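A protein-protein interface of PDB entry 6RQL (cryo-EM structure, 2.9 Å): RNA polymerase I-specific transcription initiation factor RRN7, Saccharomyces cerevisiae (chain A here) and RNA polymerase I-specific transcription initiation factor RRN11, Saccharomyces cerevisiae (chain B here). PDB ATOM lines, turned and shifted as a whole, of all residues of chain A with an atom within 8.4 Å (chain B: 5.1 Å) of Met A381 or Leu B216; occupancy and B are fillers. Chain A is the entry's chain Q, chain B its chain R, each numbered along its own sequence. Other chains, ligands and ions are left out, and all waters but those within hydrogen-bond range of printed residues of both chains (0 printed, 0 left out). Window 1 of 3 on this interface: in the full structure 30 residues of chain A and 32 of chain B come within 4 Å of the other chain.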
ATOM      1  N   THR A 187      12.367  10.922  38.255  1.00  0.00           N
ATOM      2  CA  THR A 187      11.918  12.058  37.473  1.00  0.00           C
ATOM      3  C   THR A 187      12.228  13.381  38.156  1.00  0.00           C
ATOM      4  O   THR A 187      11.827  14.433  37.646  1.00  0.00           O
ATOM      5  CB  THR A 187      10.426  11.938  37.198  1.00  0.00           C
ATOM      6  OG1 THR A 187       9.719  11.939  38.438  1.00  0.00           O
ATOM      7  CG2 THR A 187      10.148  10.640  36.491  1.00  0.00           C
ATOM      8  N   ILE A 352      11.774   7.346  32.043  1.00  0.00           N
ATOM      9  CA  ILE A 352      12.887   7.908  32.796  1.00  0.00           C
ATOM     10  C   ILE A 352      13.464   6.862  33.737  1.00  0.00           C
ATOM     11  O   ILE A 352      14.666   6.845  34.013  1.00  0.00           O
ATOM     12  CB  ILE A 352      12.426   9.147  33.581  1.00  0.00           C
ATOM     13  CG1 ILE A 352      11.563  10.068  32.728  1.00  0.00           C
ATOM     14  CG2 ILE A 352      13.618   9.922  34.073  1.00  0.00           C
ATOM     15  CD1 ILE A 352      12.232  10.639  31.560  1.00  0.00           C
ATOM     16  N   VAL A 355      15.733   4.382  31.988  1.00  0.00           N
ATOM     17  CA  VAL A 355      17.028   4.992  31.720  1.00  0.00           C
ATOM     18  C   VAL A 355      18.021   4.695  32.837  1.00  0.00           C
ATOM     19  O   VAL A 355      19.173   4.332  32.575  1.00  0.00           O
ATOM     20  CB  VAL A 355      16.826   6.503  31.516  1.00  0.00           C
ATOM     21  CG1 VAL A 355      18.112   7.257  31.657  1.00  0.00           C
ATOM     22  CG2 VAL A 355      16.219   6.764  30.152  1.00  0.00           C
ATOM     23  N   TYR A 366      15.725   3.098  24.654  1.00  0.00           N
ATOM     24  CA  TYR A 366      15.509   4.405  24.050  1.00  0.00           C
ATOM     25  C   TYR A 366      15.818   4.459  22.563  1.00  0.00           C
ATOM     26  O   TYR A 366      15.463   5.449  21.918  1.00  0.00           O
ATOM     27  CB  TYR A 366      16.325   5.458  24.791  1.00  0.00           C
ATOM     28  CG  TYR A 366      17.772   5.103  25.000  1.00  0.00           C
ATOM     29  CD1 TYR A 366      18.196   4.535  26.193  1.00  0.00           C
ATOM     30  CD2 TYR A 366      18.715   5.332  24.017  1.00  0.00           C
ATOM     31  CE1 TYR A 366      19.522   4.209  26.397  1.00  0.00           C
ATOM     32  CE2 TYR A 366      20.027   5.002  24.211  1.00  0.00           C
ATOM     33  CZ  TYR A 366      20.429   4.441  25.397  1.00  0.00           C
ATOM     34  OH  TYR A 366      21.748   4.116  25.587  1.00  0.00           O
ATOM     35  N   TRP A 369      12.444   4.426  20.748  1.00  0.00           N
ATOM     36  CA  TRP A 369      11.481   5.479  21.009  1.00  0.00           C
ATOM     37  C   TRP A 369      10.953   6.053  19.701  1.00  0.00           C
ATOM     38  O   TRP A 369      11.438   5.756  18.606  1.00  0.00           O
ATOM     39  CB  TRP A 369      12.087   6.604  21.845  1.00  0.00           C
ATOM     40  CG  TRP A 369      12.327   6.255  23.258  1.00  0.00           C
ATOM     41  CD1 TRP A 369      11.997   5.097  23.878  1.00  0.00           C
ATOM     42  CD2 TRP A 369      12.934   7.085  24.252  1.00  0.00           C
ATOM     43  NE1 TRP A 369      12.373   5.143  25.194  1.00  0.00           N
ATOM     44  CE2 TRP A 369      12.948   6.358  25.448  1.00  0.00           C
ATOM     45  CE3 TRP A 369      13.473   8.372  24.242  1.00  0.00           C
ATOM     46  CZ2 TRP A 369      13.488   6.868  26.618  1.00  0.00           C
ATOM     47  CZ3 TRP A 369      14.003   8.875  25.403  1.00  0.00           C
ATOM     48  CH2 TRP A 369      14.008   8.127  26.573  1.00  0.00           C
ATOM     49  N   THR A 374      10.425  11.317  22.378  1.00  0.00           N
ATOM     50  CA  THR A 374      11.694  11.986  22.613  1.00  0.00           C
ATOM     51  C   THR A 374      11.495  13.465  22.924  1.00  0.00           C
ATOM     52  O   THR A 374      12.209  14.019  23.764  1.00  0.00           O
ATOM     53  CB  THR A 374      12.592  11.795  21.396  1.00  0.00           C
ATOM     54  OG1 THR A 374      12.708  10.396  21.129  1.00  0.00           O
ATOM     55  CG2 THR A 374      13.978  12.329  21.650  1.00  0.00           C
ATOM     56  N   LEU A 375      10.518  14.115  22.277  1.00  0.00           N
ATOM     57  CA  LEU A 375      10.263  15.530  22.545  1.00  0.00           C
ATOM     58  C   LEU A 375       9.767  15.763  23.963  1.00  0.00           C
ATOM     59  O   LEU A 375      10.214  16.699  24.633  1.00  0.00           O
ATOM     60  CB  LEU A 375       9.258  16.111  21.555  1.00  0.00           C
ATOM     61  CG  LEU A 375       9.750  16.750  20.255  1.00  0.00           C
ATOM     62  CD1 LEU A 375      10.122  15.741  19.206  1.00  0.00           C
ATOM     63  CD2 LEU A 375       8.706  17.718  19.712  1.00  0.00           C
ATOM     64  N   GLU A 376       8.849  14.924  24.447  1.00  0.00           N
ATOM     65  CA  GLU A 376       8.406  15.069  25.827  1.00  0.00           C
ATOM     66  C   GLU A 376       9.490  14.642  26.808  1.00  0.00           C
ATOM     67  O   GLU A 376       9.517  15.135  27.940  1.00  0.00           O
ATOM     68  CB  GLU A 376       7.108  14.287  26.045  1.00  0.00           C
ATOM     69  CG  GLU A 376       6.449  14.467  27.423  1.00  0.00           C
ATOM     70  CD  GLU A 376       5.917  15.868  27.684  1.00  0.00           C
ATOM     71  OE1 GLU A 376       5.539  16.558  26.715  1.00  0.00           O
ATOM     72  OE2 GLU A 376       5.878  16.278  28.866  1.00  0.00           O
ATOM     73  N   PHE A 377      10.419  13.785  26.381  1.00  0.00           N
ATOM     74  CA  PHE A 377      11.598  13.534  27.253  1.00  0.00           C
ATOM     75  C   PHE A 377      12.439  14.814  27.302  1.00  0.00           C
ATOM     76  O   PHE A 377      12.886  15.178  28.387  1.00  0.00           O
ATOM     77  CB  PHE A 377      12.467  12.377  26.776  1.00  0.00           C
ATOM     78  CG  PHE A 377      13.606  12.055  27.709  1.00  0.00           C
ATOM     79  CD1 PHE A 377      13.409  11.266  28.828  1.00  0.00           C
ATOM     80  CD2 PHE A 377      14.877  12.545  27.474  1.00  0.00           C
ATOM     81  CE1 PHE A 377      14.454  10.960  29.681  1.00  0.00           C
ATOM     82  CE2 PHE A 377      15.921  12.241  28.330  1.00  0.00           C
ATOM     83  CZ  PHE A 377      15.707  11.451  29.431  1.00  0.00           C
ATOM     84  N   LEU A 378      12.629  15.489  26.159  1.00  0.00           N
ATOM     85  CA  LEU A 378      13.363  16.743  26.196  1.00  0.00           C
ATOM     86  C   LEU A 378      12.550  17.848  26.847  1.00  0.00           C
ATOM     87  O   LEU A 378      13.126  18.806  27.371  1.00  0.00           O
ATOM     88  CB  LEU A 378      13.766  17.147  24.785  1.00  0.00           C
ATOM     89  CG  LEU A 378      14.732  16.176  24.112  1.00  0.00           C
ATOM     90  CD1 LEU A 378      14.900  16.550  22.664  1.00  0.00           C
ATOM     91  CD2 LEU A 378      16.070  16.159  24.818  1.00  0.00           C
ATOM     92  N   LYS A 379      11.223  17.744  26.820  1.00  0.00           N
ATOM     93  CA  LYS A 379      10.403  18.638  27.627  1.00  0.00           C
ATOM     94  C   LYS A 379      10.466  18.285  29.105  1.00  0.00           C
ATOM     95  O   LYS A 379      10.217  19.149  29.950  1.00  0.00           O
ATOM     96  CB  LYS A 379       8.962  18.615  27.134  1.00  0.00           C
ATOM     97  CG  LYS A 379       8.762  19.372  25.846  1.00  0.00           C
ATOM     98  CD  LYS A 379       7.394  19.104  25.266  1.00  0.00           C
ATOM     99  CE  LYS A 379       6.307  19.724  26.113  1.00  0.00           C
ATOM    100  NZ  LYS A 379       4.974  19.514  25.488  1.00  0.00           N
ATOM    101  N   TRP A 380      10.787  17.037  29.438  1.00  0.00           N
ATOM    102  CA  TRP A 380      11.110  16.727  30.823  1.00  0.00           C
ATOM    103  C   TRP A 380      12.455  17.314  31.221  1.00  0.00           C
ATOM    104  O   TRP A 380      12.638  17.705  32.379  1.00  0.00           O
ATOM    105  CB  TRP A 380      11.110  15.219  31.049  1.00  0.00           C
ATOM    106  CG  TRP A 380      11.546  14.885  32.419  1.00  0.00           C
ATOM    107  CD1 TRP A 380      10.874  15.128  33.574  1.00  0.00           C
ATOM    108  CD2 TRP A 380      12.803  14.336  32.795  1.00  0.00           C
ATOM    109  NE1 TRP A 380      11.617  14.722  34.647  1.00  0.00           N
ATOM    110  CE2 TRP A 380      12.811  14.231  34.190  1.00  0.00           C
ATOM    111  CE3 TRP A 380      13.918  13.903  32.083  1.00  0.00           C
ATOM    112  CZ2 TRP A 380      13.888  13.710  34.887  1.00  0.00           C
ATOM    113  CZ3 TRP A 380      14.979  13.382  32.775  1.00  0.00           C
ATOM    114  CH2 TRP A 380      14.961  13.291  34.160  1.00  0.00           C
ATOM    115  N   MET A 381      13.383  17.427  30.263  1.00  0.00           N
ATOM    116  CA  MET A 381      14.743  17.889  30.532  1.00  0.00           C
ATOM    117  C   MET A 381      14.806  19.317  31.050  1.00  0.00           C
ATOM    118  O   MET A 381      15.805  19.695  31.664  1.00  0.00           O
ATOM    119  CB  MET A 381      15.592  17.778  29.271  1.00  0.00           C
ATOM    120  CG  MET A 381      15.936  16.369  28.870  1.00  0.00           C
ATOM    121  SD  MET A 381      16.980  15.588  30.083  1.00  0.00           S
ATOM    122  CE  MET A 381      18.426  16.599  29.859  1.00  0.00           C
ATOM    123  N   GLU A 382      13.754  20.102  30.857  1.00  0.00           N
ATOM    124  CA  GLU A 382      13.596  21.381  31.529  1.00  0.00           C
ATOM    125  C   GLU A 382      13.128  21.244  32.987  1.00  0.00           C
ATOM    126  O   GLU A 382      12.748  22.244  33.599  1.00  0.00           O
ATOM    127  CB  GLU A 382      12.621  22.248  30.739  1.00  0.00           C
ATOM    128  CG  GLU A 382      13.130  22.604  29.358  1.00  0.00           C
ATOM    129  CD  GLU A 382      12.106  23.368  28.557  1.00  0.00           C
ATOM    130  OE1 GLU A 382      10.957  23.484  29.033  1.00  0.00           O
ATOM    131  OE2 GLU A 382      12.444  23.851  27.459  1.00  0.00           O
ATOM    132  N   LYS A 383      13.113  20.028  33.541  1.00  0.00           N
ATOM    133  CA  LYS A 383      13.054  19.822  34.979  1.00  0.00           C
ATOM    134  C   LYS A 383      14.267  19.010  35.441  1.00  0.00           C
ATOM    135  O   LYS A 383      14.342  18.614  36.607  1.00  0.00           O
ATOM    136  CB  LYS A 383      11.723  19.152  35.379  1.00  0.00           C
ATOM    137  CG  LYS A 383      11.321  19.274  36.872  1.00  0.00           C
ATOM    138  CD  LYS A 383      10.072  18.514  37.224  1.00  0.00           C
ATOM    139  CE  LYS A 383       8.839  19.285  36.851  1.00  0.00           C
ATOM    140  NZ  LYS A 383       8.683  20.468  37.746  1.00  0.00           N
ATOM    141  N   GLN A 384      15.242  18.761  34.569  1.00  0.00           N
ATOM    142  CA  GLN A 384      16.489  18.244  35.117  1.00  0.00           C
ATOM    143  C   GLN A 384      17.471  19.360  35.450  1.00  0.00           C
ATOM    144  O   GLN A 384      18.124  19.308  36.499  1.00  0.00           O
ATOM    145  CB  GLN A 384      17.155  17.241  34.171  1.00  0.00           C
ATOM    146  CG  GLN A 384      18.392  16.611  34.817  1.00  0.00           C
ATOM    147  CD  GLN A 384      19.114  15.619  33.957  1.00  0.00           C
ATOM    148  OE1 GLN A 384      18.711  15.349  32.841  1.00  0.00           O
ATOM    149  NE2 GLN A 384      20.209  15.081  34.471  1.00  0.00           N
ATOM    150  N   PHE A 385      17.565  20.394  34.609  1.00  0.00           N
ATOM    151  CA  PHE A 385      18.608  21.393  34.807  1.00  0.00           C
ATOM    152  C   PHE A 385      18.340  22.294  35.998  1.00  0.00           C
ATOM    153  O   PHE A 385      19.267  22.947  36.483  1.00  0.00           O
ATOM    154  CB  PHE A 385      18.774  22.288  33.587  1.00  0.00           C
ATOM    155  CG  PHE A 385      18.886  21.550  32.307  1.00  0.00           C
ATOM    156  CD1 PHE A 385      19.883  20.616  32.116  1.00  0.00           C
ATOM    157  CD2 PHE A 385      18.055  21.871  31.256  1.00  0.00           C
ATOM    158  CE1 PHE A 385      19.989  19.953  30.928  1.00  0.00           C
ATOM    159  CE2 PHE A 385      18.163  21.223  30.066  1.00  0.00           C
ATOM    160  CZ  PHE A 385      19.131  20.263  29.899  1.00  0.00           C
ATOM    161  N   LEU A 386      17.113  22.363  36.462  1.00  0.00           N
ATOM    162  CA  LEU A 386      16.852  23.233  37.595  1.00  0.00           C
ATOM    163  C   LEU A 386      17.307  22.581  38.905  1.00  0.00           C
ATOM    164  O   LEU A 386      17.843  23.295  39.761  1.00  0.00           O
ATOM    165  CB  LEU A 386      15.381  23.661  37.631  1.00  0.00           C
ATOM    166  CG  LEU A 386      14.954  24.783  36.679  1.00  0.00           C
ATOM    167  CD1 LEU A 386      14.750  24.301  35.247  1.00  0.00           C
ATOM    168  CD2 LEU A 386      13.707  25.493  37.195  1.00  0.00           C
ATOM    169  N   PRO A 387      17.136  21.243  39.133  1.00  0.00           N
ATOM    170  CA  PRO A 387      17.937  20.614  40.193  1.00  0.00           C
ATOM    171  C   PRO A 387      19.412  20.535  39.853  1.00  0.00           C
ATOM    172  O   PRO A 387      20.260  20.763  40.718  1.00  0.00           O
ATOM    173  CB  PRO A 387      17.325  19.216  40.319  1.00  0.00           C
ATOM    174  CG  PRO A 387      15.956  19.384  39.893  1.00  0.00           C
ATOM    175  CD  PRO A 387      16.001  20.366  38.781  1.00  0.00           C
ATOM    176  N   THR A 388      19.732  20.217  38.605  1.00  0.00           N
ATOM    177  CA  THR A 388      21.118  19.997  38.209  1.00  0.00           C
ATOM    178  C   THR A 388      21.664  21.110  37.313  1.00  0.00           C
ATOM    179  O   THR A 388      22.340  22.028  37.773  1.00  0.00           O
ATOM    180  CB  THR A 388      21.262  18.659  37.474  1.00  0.00           C
ATOM    181  OG1 THR A 388      20.795  17.600  38.315  1.00  0.00           O
ATOM    182  CG2 THR A 388      22.706  18.412  37.112  1.00  0.00           C
ATOM    183  N   LEU A 419      18.034  27.609  24.455  1.00  0.00           N
ATOM    184  CA  LEU A 419      17.427  26.362  24.899  1.00  0.00           C
ATOM    185  C   LEU A 419      16.057  26.158  24.280  1.00  0.00           C
ATOM    186  O   LEU A 419      15.616  25.013  24.132  1.00  0.00           O
ATOM    187  CB  LEU A 419      17.360  26.334  26.427  1.00  0.00           C
ATOM    188  CG  LEU A 419      17.101  25.024  27.181  1.00  0.00           C
ATOM    189  CD1 LEU A 419      15.633  24.698  27.397  1.00  0.00           C
ATOM    190  CD2 LEU A 419      17.771  23.887  26.439  1.00  0.00           C
ATOM    191  N   HIS B 212      22.151   9.709  32.266  1.00  0.00           N
ATOM    192  CA  HIS B 212      21.412  10.472  31.269  1.00  0.00           C
ATOM    193  C   HIS B 212      22.296  11.056  30.182  1.00  0.00           C
ATOM    194  O   HIS B 212      21.789  11.372  29.105  1.00  0.00           O
ATOM    195  CB  HIS B 212      20.613  11.597  31.930  1.00  0.00           C
ATOM    196  CG  HIS B 212      19.337  11.134  32.555  1.00  0.00           C
ATOM    197  ND1 HIS B 212      19.281  10.579  33.814  1.00  0.00           N
ATOM    198  CD2 HIS B 212      18.065  11.153  32.095  1.00  0.00           C
ATOM    199  CE1 HIS B 212      18.030  10.264  34.098  1.00  0.00           C
ATOM    200  NE2 HIS B 212      17.273  10.604  33.072  1.00  0.00           N
ATOM    201  N   ILE B 213      23.596  11.204  30.434  1.00  0.00           N
ATOM    202  CA  ILE B 213      24.514  11.599  29.372  1.00  0.00           C
ATOM    203  C   ILE B 213      24.662  10.479  28.354  1.00  0.00           C
ATOM    204  O   ILE B 213      24.662  10.725  27.144  1.00  0.00           O
ATOM    205  CB  ILE B 213      25.864  12.023  29.975  1.00  0.00           C
ATOM    206  CG1 ILE B 213      25.705  13.332  30.733  1.00  0.00           C
ATOM    207  CG2 ILE B 213      26.917  12.199  28.909  1.00  0.00           C
ATOM    208  CD1 ILE B 213      26.887  13.672  31.565  1.00  0.00           C
ATOM    209  N   VAL B 214      24.747   9.230  28.823  1.00  0.00           N
ATOM    210  CA  VAL B 214      24.778   8.082  27.918  1.00  0.00           C
ATOM    211  C   VAL B 214      23.463   7.977  27.160  1.00  0.00           C
ATOM    212  O   VAL B 214      23.429   7.611  25.979  1.00  0.00           O
ATOM    213  CB  VAL B 214      25.089   6.797  28.710  1.00  0.00           C
ATOM    214  CG1 VAL B 214      25.061   5.574  27.824  1.00  0.00           C
ATOM    215  CG2 VAL B 214      26.437   6.905  29.346  1.00  0.00           C
ATOM    216  N   THR B 215      22.374   8.369  27.807  1.00  0.00           N
ATOM    217  CA  THR B 215      21.074   8.361  27.155  1.00  0.00           C
ATOM    218  C   THR B 215      20.980   9.454  26.102  1.00  0.00           C
ATOM    219  O   THR B 215      20.461   9.229  25.008  1.00  0.00           O
ATOM    220  CB  THR B 215      19.992   8.523  28.208  1.00  0.00           C
ATOM    221  OG1 THR B 215      20.184   7.512  29.195  1.00  0.00           O
ATOM    222  CG2 THR B 215      18.630   8.350  27.598  1.00  0.00           C
ATOM    223  N   LEU B 216      21.509  10.639  26.397  1.00  0.00           N
ATOM    224  CA  LEU B 216      21.382  11.741  25.457  1.00  0.00           C
ATOM    225  C   LEU B 216      22.333  11.645  24.276  1.00  0.00           C
ATOM    226  O   LEU B 216      21.946  12.033  23.172  1.00  0.00           O
ATOM    227  CB  LEU B 216      21.602  13.069  26.161  1.00  0.00           C
ATOM    228  CG  LEU B 216      20.438  13.516  27.020  1.00  0.00           C
ATOM    229  CD1 LEU B 216      20.831  14.757  27.737  1.00  0.00           C
ATOM    230  CD2 LEU B 216      19.235  13.766  26.148  1.00  0.00           C
ATOM    231  N   THR B 217      23.564  11.172  24.469  1.00  0.00           N
ATOM    232  CA  THR B 217      24.473  11.092  23.331  1.00  0.00           C
ATOM    233  C   THR B 217      24.117   9.959  22.395  1.00  0.00           C
ATOM    234  O   THR B 217      24.358  10.066  21.191  1.00  0.00           O
ATOM    235  CB  THR B 217      25.916  10.917  23.788  1.00  0.00           C
ATOM    236  OG1 THR B 217      26.039   9.684  24.499  1.00  0.00           O
ATOM    237  CG2 THR B 217      26.315  12.051  24.676  1.00  0.00           C
ATOM    238  N   ASP B 218      23.546   8.879  22.916  1.00  0.00           N
ATOM    239  CA  ASP B 218      23.096   7.826  22.025  1.00  0.00           C
ATOM    240  C   ASP B 218      21.845   8.211  21.251  1.00  0.00           C
ATOM    241  O   ASP B 218      21.619   7.660  20.177  1.00  0.00           O
ATOM    242  CB  ASP B 218      22.845   6.543  22.809  1.00  0.00           C
ATOM    243  CG  ASP B 218      24.124   5.855  23.225  1.00  0.00           C
ATOM    244  OD1 ASP B 218      25.131   5.981  22.507  1.00  0.00           O
ATOM    245  OD2 ASP B 218      24.122   5.169  24.269  1.00  0.00           O
ATOM    246  N   LEU B 219      21.039   9.149  21.755  1.00  0.00           N
ATOM    247  CA  LEU B 219      19.943   9.678  20.953  1.00  0.00           C
ATOM    248  C   LEU B 219      20.407  10.796  20.042  1.00  0.00           C
ATOM    249  O   LEU B 219      19.739  11.105  19.052  1.00  0.00           O
ATOM    250  CB  LEU B 219      18.830  10.221  21.843  1.00  0.00           C
ATOM    251  CG  LEU B 219      18.097   9.253  22.744  1.00  0.00           C
ATOM    252  CD1 LEU B 219      17.082  10.022  23.548  1.00  0.00           C
ATOM    253  CD2 LEU B 219      17.458   8.161  21.932  1.00  0.00           C
ATOM    254  N   LEU B 220      21.523  11.429  20.387  1.00  0.00           N
ATOM    255  CA  LEU B 220      22.041  12.524  19.585  1.00  0.00           C
ATOM    256  C   LEU B 220      22.652  12.016  18.296  1.00  0.00           C
ATOM    257  O   LEU B 220      22.306  12.488  17.210  1.00  0.00           O
ATOM    258  CB  LEU B 220      23.072  13.301  20.381  1.00  0.00           C
ATOM    259  CG  LEU B 220      23.772  14.436  19.661  1.00  0.00           C
ATOM    260  CD1 LEU B 220      22.770  15.420  19.142  1.00  0.00           C
ATOM    261  CD2 LEU B 220      24.634  15.095  20.680  1.00  0.00           C
ATOM    262  N   ILE B 235      18.460  18.029  21.407  1.00  0.00           N
ATOM    263  CA  ILE B 235      19.264  17.145  22.238  1.00  0.00           C
ATOM    264  C   ILE B 235      20.600  17.795  22.548  1.00  0.00           C
ATOM    265  O   ILE B 235      21.074  17.765  23.688  1.00  0.00           O
ATOM    266  CB  ILE B 235      19.450  15.789  21.542  1.00  0.00           C
ATOM    267  CG1 ILE B 235      18.103  15.137  21.289  1.00  0.00           C
ATOM    268  CG2 ILE B 235      20.289  14.871  22.387  1.00  0.00           C
ATOM    269  CD1 ILE B 235      18.183  13.951  20.395  1.00  0.00           C
ATOM    270  N   THR B 238      20.418  20.633  25.054  1.00  0.00           N
ATOM    271  CA  THR B 238      20.210  20.085  26.383  1.00  0.00           C
ATOM    272  C   THR B 238      21.352  19.205  26.851  1.00  0.00           C
ATOM    273  O   THR B 238      21.340  18.762  28.002  1.00  0.00           O
ATOM    274  CB  THR B 238      18.922  19.272  26.423  1.00  0.00           C
ATOM    275  OG1 THR B 238      18.943  18.319  25.362  1.00  0.00           O
ATOM    276  CG2 THR B 238      17.719  20.165  26.278  1.00  0.00           C
ATOM    277  N   LEU B 239      22.320  18.927  25.994  1.00  0.00           N
ATOM    278  CA  LEU B 239      23.461  18.124  26.399  1.00  0.00           C
ATOM    279  C   LEU B 239      24.581  18.980  26.956  1.00  0.00           C
ATOM    280  O   LEU B 239      25.222  18.600  27.936  1.00  0.00           O
ATOM    281  CB  LEU B 239      23.967  17.308  25.215  1.00  0.00           C
ATOM    282  CG  LEU B 239      25.128  16.372  25.493  1.00  0.00           C
ATOM    283  CD1 LEU B 239      24.722  15.377  26.536  1.00  0.00           C
ATOM    284  CD2 LEU B 239      25.519  15.675  24.229  1.00  0.00           C
ATOM    285  N   ILE B 242      24.417  20.160  30.784  1.00  0.00           N
ATOM    286  CA  ILE B 242      24.682  19.268  31.912  1.00  0.00           C
ATOM    287  C   ILE B 242      26.117  19.492  32.375  1.00  0.00           C
ATOM    288  O   ILE B 242      27.019  19.576  31.531  1.00  0.00           O
ATOM    289  CB  ILE B 242      24.461  17.822  31.494  1.00  0.00           C
ATOM    290  CG1 ILE B 242      23.024  17.632  31.053  1.00  0.00           C
ATOM    291  CG2 ILE B 242      24.771  16.857  32.612  1.00  0.00           C
ATOM    292  CD1 ILE B 242      22.800  16.333  30.409  1.00  0.00           C
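OD2 of Asp B218 sits at hydrogen-bond distance from OH of Tyr A366 (2.9 Å).
The indole nitrogen (NE1) of Trp A380 lies within hydrogen-bond range of the backbone carbonyl oxygen (O) of Thr A187 (3.0 Å). SD of Met A381 sits close to OE1 of Gln A384, at 3.3 Å. The backbone carbonyl oxygen (O) of Ile B235 lies within hydrogen-bond range of the side-chain hydroxyl (OG1) of Thr B238, at 2.8 Å.
Among the printed residues, pairs that only touch across the chains: Val A355 with Thr B215, Phe A385 with Thr B238, Tyr A366 with Leu B219, Phe A377 with His B212, Trp A380 with His B212, Leu A378 with Thr B238, Met A381 with Leu B216, Leu A419 with Thr B238, Val A355 with His B212, Leu A378 with Ile B235, Trp A369 with Leu B219, Phe A385 with Ile B242, Ile A352 with His B212 and Tyr A366 with Val B214.
Of the printed residues of chain B, Met A381 touches Leu B216 (3.7 Å). Of the printed residues of chain A, Leu B216 touches Met A381 (3.7 Å). No residue of chain A comes within 4 Å of Thr B217. Of the printed residues of chain B, Ile A352 touches His B212. Printed residues of chain A within 4 Å of Val B214: Tyr A366. Of the printed residues of chain B, Leu A419 touches Thr B238 (3.7 Å). Thr A388 touches none of the printed residues of chain B. Leu B239 touches none of the printed residues of chain A. The nearest residue of chain B that does not touch Met A381 is Thr B238 (4.1 Å). The nearest printed residue of chain A that does not touch Ile B235 is Thr A374 (4.7 Å).
Hydrophobic or aromatic side chains of chain B within 4 Å of the printed part of chain A: His B212, Leu B216, Leu B219, Ile B235 and Ile B242. Hydrophobic or aromatic side chains of chain A that line the printed part of chain B: Ile A352, Val A355, Tyr A366, Trp A369, Phe A377, Leu A378, Trp A380, Met A381, Phe A385 and Leu A419. Along chain A the printed residues that touch a printed residue of chain B span positions 352 to 419. Among the printed residues, 15 pairs touch across the chains.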
